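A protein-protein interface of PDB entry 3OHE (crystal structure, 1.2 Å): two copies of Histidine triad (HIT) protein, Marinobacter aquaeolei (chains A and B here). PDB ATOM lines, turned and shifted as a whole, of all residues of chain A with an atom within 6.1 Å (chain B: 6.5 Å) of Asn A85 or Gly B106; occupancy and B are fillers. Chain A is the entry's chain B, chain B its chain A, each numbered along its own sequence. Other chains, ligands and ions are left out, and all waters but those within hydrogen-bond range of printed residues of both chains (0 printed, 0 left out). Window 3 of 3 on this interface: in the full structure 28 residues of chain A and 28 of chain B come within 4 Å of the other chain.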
ATOM      1  N   LEU A  83     -26.369 -13.101  -1.228  1.00  0.00           N
ATOM      2  CA  LEU A  83     -27.271 -12.012  -0.810  1.00  0.00           C
ATOM      3  C   LEU A  83     -26.436 -10.733  -0.696  1.00  0.00           C
ATOM      4  O   LEU A  83     -26.372  -9.928  -1.640  1.00  0.00           O
ATOM      5  CB  LEU A  83     -28.028 -12.413   0.477  1.00  0.00           C
ATOM      6  CG  LEU A  83     -28.828 -13.727   0.387  1.00  0.00           C
ATOM      7  CD1 LEU A  83     -29.447 -14.059   1.731  1.00  0.00           C
ATOM      8  CD2 LEU A  83     -29.891 -13.688  -0.734  1.00  0.00           C
ATOM      9  N   GLY A  84     -25.754 -10.536   0.426  1.00  0.00           N
ATOM     10  CA  GLY A  84     -24.762  -9.474   0.542  1.00  0.00           C
ATOM     11  C   GLY A  84     -25.303  -8.070   0.640  1.00  0.00           C
ATOM     12  O   GLY A  84     -24.655  -7.122   0.223  1.00  0.00           O
ATOM     13  N   ASN A  85     -26.458  -7.906   1.255  1.00  0.00           N
ATOM     14  CA  ASN A  85     -27.007  -6.562   1.383  1.00  0.00           C
ATOM     15  C   ASN A  85     -26.258  -5.681   2.377  1.00  0.00           C
ATOM     16  O   ASN A  85     -26.233  -4.465   2.204  1.00  0.00           O
ATOM     17  CB  ASN A  85     -28.470  -6.627   1.773  1.00  0.00           C
ATOM     18  CG  ASN A  85     -29.315  -7.342   0.756  1.00  0.00           C
ATOM     19  OD1 ASN A  85     -29.021  -7.362  -0.420  1.00  0.00           O
ATOM     20  ND2 ASN A  85     -30.416  -7.890   1.228  1.00  0.00           N
ATOM     21  N   MET A  86     -25.675  -6.321   3.385  1.00  0.00           N
ATOM     22  CA  MET A  86     -24.876  -5.656   4.452  1.00  0.00           C
ATOM     23  C   MET A  86     -23.370  -5.706   4.198  1.00  0.00           C
ATOM     24  O   MET A  86     -22.642  -4.757   4.496  1.00  0.00           O
ATOM     25  CB  MET A  86     -25.181  -6.280   5.813  1.00  0.00           C
ATOM     26  CG  MET A  86     -26.579  -5.934   6.232  1.00  0.00           C
ATOM     27  SD  MET A  86     -27.290  -6.752   7.820  1.00  0.00           S
ATOM     28  CE  MET A  86     -26.836  -8.611   7.423  1.00  0.00           C
ATOM     29  N   VAL A  87     -22.910  -6.824   3.660  1.00  0.00           N
ATOM     30  CA  VAL A  87     -21.499  -7.108   3.461  1.00  0.00           C
ATOM     31  C   VAL A  87     -21.254  -7.193   1.946  1.00  0.00           C
ATOM     32  O   VAL A  87     -21.776  -8.118   1.300  1.00  0.00           O
ATOM     33  CB  VAL A  87     -21.090  -8.419   4.145  1.00  0.00           C
ATOM     34  CG1 VAL A  87     -19.654  -8.820   3.715  1.00  0.00           C
ATOM     35  CG2 VAL A  87     -21.210  -8.269   5.655  1.00  0.00           C
ATOM     36  N   PRO A  88     -20.504  -6.246   1.374  1.00  0.00           N
ATOM     37  CA  PRO A  88     -20.414  -6.151  -0.087  1.00  0.00           C
ATOM     38  C   PRO A  88     -19.500  -7.199  -0.726  1.00  0.00           C
ATOM     39  O   PRO A  88     -19.620  -7.439  -1.913  1.00  0.00           O
ATOM     40  CB  PRO A  88     -19.869  -4.730  -0.294  1.00  0.00           C
ATOM     41  CG  PRO A  88     -19.018  -4.466   0.904  1.00  0.00           C
ATOM     42  CD  PRO A  88     -19.819  -5.092   2.011  1.00  0.00           C
ATOM     43  N   LYS B  77     -28.202  -3.921  -5.383  1.00  0.00           N
ATOM     44  CA  LYS B  77     -27.595  -5.202  -5.056  1.00  0.00           C
ATOM     45  C   LYS B  77     -28.500  -6.299  -5.609  1.00  0.00           C
ATOM     46  O   LYS B  77     -29.692  -6.175  -5.563  1.00  0.00           O
ATOM     47  CB  LYS B  77     -27.460  -5.352  -3.544  1.00  0.00           C
ATOM     48  CG  LYS B  77     -26.662  -6.547  -3.075  1.00  0.00           C
ATOM     49  CD  LYS B  77     -25.169  -6.459  -3.441  1.00  0.00           C
ATOM     50  CE  LYS B  77     -24.375  -7.772  -3.157  1.00  0.00           C
ATOM     51  NZ  LYS B  77     -24.981  -8.954  -3.874  1.00  0.00           N
ATOM     52  N   MET B  78     -27.882  -7.372  -6.116  1.00  0.00           N
ATOM     53  CA  MET B  78     -28.647  -8.567  -6.451  1.00  0.00           C
ATOM     54  C   MET B  78     -28.713  -9.540  -5.319  1.00  0.00           C
ATOM     55  O   MET B  78     -27.786  -9.647  -4.516  1.00  0.00           O
ATOM     56  CB  MET B  78     -28.039  -9.305  -7.654  1.00  0.00           C
ATOM     57  CG  MET B  78     -28.148  -8.541  -8.936  1.00  0.00           C
ATOM     58  SD  MET B  78     -29.978  -8.154  -9.519  1.00  0.00           S
ATOM     59  CE  MET B  78     -30.786  -9.850  -9.755  1.00  0.00           C
ATOM     60  N   ASN B  79     -29.823 -10.263  -5.267  1.00  0.00           N
ATOM     61  CA  ASN B  79     -29.936 -11.446  -4.393  1.00  0.00           C
ATOM     62  C   ASN B  79     -30.299 -12.638  -5.299  1.00  0.00           C
ATOM     63  O   ASN B  79     -31.277 -12.566  -6.053  1.00  0.00           O
ATOM     64  CB  ASN B  79     -31.004 -11.267  -3.337  1.00  0.00           C
ATOM     65  CG  ASN B  79     -30.692 -10.246  -2.236  1.00  0.00           C
ATOM     66  OD1 ASN B  79     -31.576 -10.071  -1.373  1.00  0.00           O
ATOM     67  ND2 ASN B  79     -29.522  -9.622  -2.211  1.00  0.00           N
ATOM     68  N   ARG B  97     -32.487  -5.606  -5.467  1.00  0.00           N
ATOM     69  CA  ARG B  97     -32.697  -4.925  -4.191  1.00  0.00           C
ATOM     70  C   ARG B  97     -32.251  -3.468  -4.261  1.00  0.00           C
ATOM     71  O   ARG B  97     -31.343  -3.117  -5.039  1.00  0.00           O
ATOM     72  CB  ARG B  97     -31.896  -5.622  -3.069  1.00  0.00           C
ATOM     73  CG  ARG B  97     -32.193  -7.086  -2.915  1.00  0.00           C
ATOM     74  CD  ARG B  97     -33.645  -7.385  -2.594  1.00  0.00           C
ATOM     75  NE  ARG B  97     -34.094  -6.674  -1.395  1.00  0.00           N
ATOM     76  CZ  ARG B  97     -33.950  -7.118  -0.159  1.00  0.00           C
ATOM     77  NH1 ARG B  97     -33.378  -8.266   0.089  1.00  0.00           N
ATOM     78  NH2 ARG B  97     -34.374  -6.378   0.859  1.00  0.00           N
ATOM     79  N   ASP B 101     -35.844  -0.180  -0.535  1.00  0.00           N
ATOM     80  CA  ASP B 101     -36.923  -1.188  -0.602  1.00  0.00           C
ATOM     81  C   ASP B 101     -37.458  -1.594   0.779  1.00  0.00           C
ATOM     82  O   ASP B 101     -36.826  -1.341   1.807  1.00  0.00           O
ATOM     83  CB  ASP B 101     -36.593  -2.406  -1.519  1.00  0.00           C
ATOM     84  CG  ASP B 101     -35.631  -3.433  -0.913  1.00  0.00           C
ATOM     85  OD1 ASP B 101     -35.720  -3.746   0.288  1.00  0.00           O
ATOM     86  OD2 ASP B 101     -34.802  -3.990  -1.684  1.00  0.00           O
ATOM     87  N   ALA B 103     -37.793  -4.270   2.481  1.00  0.00           N
ATOM     88  CA  ALA B 103     -37.226  -5.379   3.245  1.00  0.00           C
ATOM     89  C   ALA B 103     -35.816  -5.111   3.697  1.00  0.00           C
ATOM     90  O   ALA B 103     -35.278  -5.883   4.524  1.00  0.00           O
ATOM     91  CB  ALA B 103     -37.269  -6.687   2.454  1.00  0.00           C
ATOM     92  N   TRP B 104     -35.212  -4.061   3.151  1.00  0.00           N
ATOM     93  CA  TRP B 104     -33.783  -3.839   3.258  1.00  0.00           C
ATOM     94  C   TRP B 104     -33.404  -3.618   4.704  1.00  0.00           C
ATOM     95  O   TRP B 104     -34.206  -3.082   5.495  1.00  0.00           O
ATOM     96  CB  TRP B 104     -33.337  -2.640   2.410  1.00  0.00           C
ATOM     97  CG  TRP B 104     -31.847  -2.377   2.351  1.00  0.00           C
ATOM     98  CD1 TRP B 104     -31.105  -1.554   3.186  1.00  0.00           C
ATOM     99  CD2 TRP B 104     -30.926  -2.885   1.387  1.00  0.00           C
ATOM    100  NE1 TRP B 104     -29.804  -1.533   2.781  1.00  0.00           N
ATOM    101  CE2 TRP B 104     -29.654  -2.349   1.692  1.00  0.00           C
ATOM    102  CE3 TRP B 104     -31.044  -3.753   0.312  1.00  0.00           C
ATOM    103  CZ2 TRP B 104     -28.541  -2.637   0.953  1.00  0.00           C
ATOM    104  CZ3 TRP B 104     -29.933  -4.037  -0.419  1.00  0.00           C
ATOM    105  CH2 TRP B 104     -28.690  -3.486  -0.094  1.00  0.00           C
ATOM    106  N   PRO B 105     -32.204  -4.077   5.084  1.00  0.00           N
ATOM    107  CA  PRO B 105     -31.292  -4.979   4.396  1.00  0.00           C
ATOM    108  C   PRO B 105     -31.539  -6.495   4.562  1.00  0.00           C
ATOM    109  O   PRO B 105     -30.672  -7.296   4.171  1.00  0.00           O
ATOM    110  CB  PRO B 105     -29.964  -4.593   5.016  1.00  0.00           C
ATOM    111  CG  PRO B 105     -30.311  -4.474   6.439  1.00  0.00           C
ATOM    112  CD  PRO B 105     -31.666  -3.728   6.414  1.00  0.00           C
ATOM    113  N   GLY B 106     -32.669  -6.914   5.111  1.00  0.00           N
ATOM    114  CA  GLY B 106     -32.999  -8.312   5.231  1.00  0.00           C
ATOM    115  C   GLY B 106     -33.470  -8.975   3.941  1.00  0.00           C
ATOM    116  O   GLY B 106     -33.631  -8.305   2.915  1.00  0.00           O
ATOM    117  N   PRO B 107     -33.715 -10.294   3.989  1.00  0.00           N
ATOM    118  CA  PRO B 107     -34.212 -11.012   2.835  1.00  0.00           C
ATOM    119  C   PRO B 107     -35.677 -10.672   2.564  1.00  0.00           C
ATOM    120  O   PRO B 107     -36.402 -10.219   3.471  1.00  0.00           O
ATOM    121  CB  PRO B 107     -34.065 -12.479   3.248  1.00  0.00           C
ATOM    122  CG  PRO B 107     -34.066 -12.466   4.774  1.00  0.00           C
ATOM    123  CD  PRO B 107     -33.481 -11.181   5.167  1.00  0.00           C
ATOM    124  N   VAL B 108     -36.112 -10.889   1.330  1.00  0.00           N
ATOM    125  CA  VAL B 108     -37.474 -10.573   0.958  1.00  0.00           C
ATOM    126  C   VAL B 108     -38.478 -11.640   1.340  1.00  0.00           C
ATOM    127  O   VAL B 108     -39.660 -11.310   1.574  1.00  0.00           O
ATOM    128  CB  VAL B 108     -37.610 -10.252  -0.557  1.00  0.00           C
ATOM    129  CG1 VAL B 108     -36.621  -9.147  -0.987  1.00  0.00           C
ATOM    130  CG2 VAL B 108     -37.517 -11.497  -1.422  1.00  0.00           C
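No position is printed for both chains.
The side-chain carboxylate (OD1) of Asp B101 lies within hydrogen-bond range of the backbone NH (N) of Trp B104 (2.9 Å).
The guanidinium group (NH1) of Arg B97 lies within hydrogen-bond range of the backbone carbonyl oxygen (O) of Gly B106.
The backbone NH of Arg B97 sits at hydrogen-bond distance from the backbone carbonyl oxygen of Lys B77 (2.9 Å).
OD1 of Asn B79 sits at hydrogen-bond distance from NH1 of Arg B97 (2.9 Å).
The guanidinium group (NE) of Arg B97 is in salt-bridge range of the side-chain carboxylate (OD2) of Asp B101 (2.8 Å).
Of the printed residues of chain B, Asn A85 touches Lys B77 (3.6 Å), Asn B79 (2.9 Å), Arg B97 (3.2 Å), Trp B104 (3.2 Å), Pro B105 (3.0 Å) and Gly B106 (3.7 Å).
Gly B106 touches just one residue of chain A: Asn A85.
Printed residues of chain A within 4 Å of Pro B105: Asn A85 and Met A86.
Printed residues of chain A within 4 Å of Trp B104: Asn A85.
Printed residues of chain B within 4 Å of Leu A83: Lys B77 (2.8 Å), Met B78 (3.2 Å) and Asn B79 (3.2 Å).
Printed residues of chain B within 4 Å of Gly A84: Lys B77 (3.5 Å).
Of the printed residues of chain A, Arg B97 touches Asn A85.
Asp B101 touches none of the printed residues of chain A.
The nearest printed residue of chain B that does not touch Asn A85 is Met B78 (4.9 Å).
The nearest printed residue of chain B that does not touch Gly A84 is Asn B79 (4.7 Å).
Printed residues of chain B that touch a printed residue of chain A: Lys B77, Met B78, Asn B79, Arg B97, Trp B104, Pro B105 and Gly B106.
Hydrophobic or aromatic side chains of chain B within 4 Å of the printed part of chain A: Trp B104 and Pro B105.
Of the 6 printed residues of chain A, 4 touch a printed residue of chain B.
Hydrophobic or aromatic side chains of chain A within 4 Å of the printed part of chain B: Leu A83 and Met A86.
Along chain A the printed residues that touch a printed residue of chain B span positions 83 to 86.
Among the printed residues, 11 pairs touch across the chains.
Among the printed residues, no Asp or Glu carboxylate lies within 4 Å of a Lys or Arg side-chain nitrogen of the other chain.
The side-chain amide nitrogen (ND2) of Asn B79 lies within hydrogen-bond range of the side-chain amide oxygen (OD1) of Asn A85 (2.9 Å).
The guanidinium group (NH1) of Arg B97 sits close to the side-chain amide nitrogen (ND2) of Asn A85, at 3.2 Å.
O of Leu A83 lies close to O of Met B78, at 3.2 Å.
The side-chain amino group (NZ) of Lys B77 lies within hydrogen-bond range of the backbone carbonyl oxygen (O) of Leu A83 (2.8 Å).
The side-chain amide nitrogen (ND2) of Asn B79 lies within hydrogen-bond range of the backbone carbonyl oxygen (O) of Leu A83 (3.2 Å).
ND2 of Asn A85 is in hydrogen-bond range of O of Pro B105, at 3.0 Å.
Among the printed residues, pairs that only touch across the chains: Asn A85 with Trp B104 (3.2 Å), Gly A84 with Lys B77 (3.5 Å), Asn A85 with Lys B77 (3.6 Å), Asn A85 with Gly B106 (3.7 Å) and Met A86 with Pro B105 (3.8 Å).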
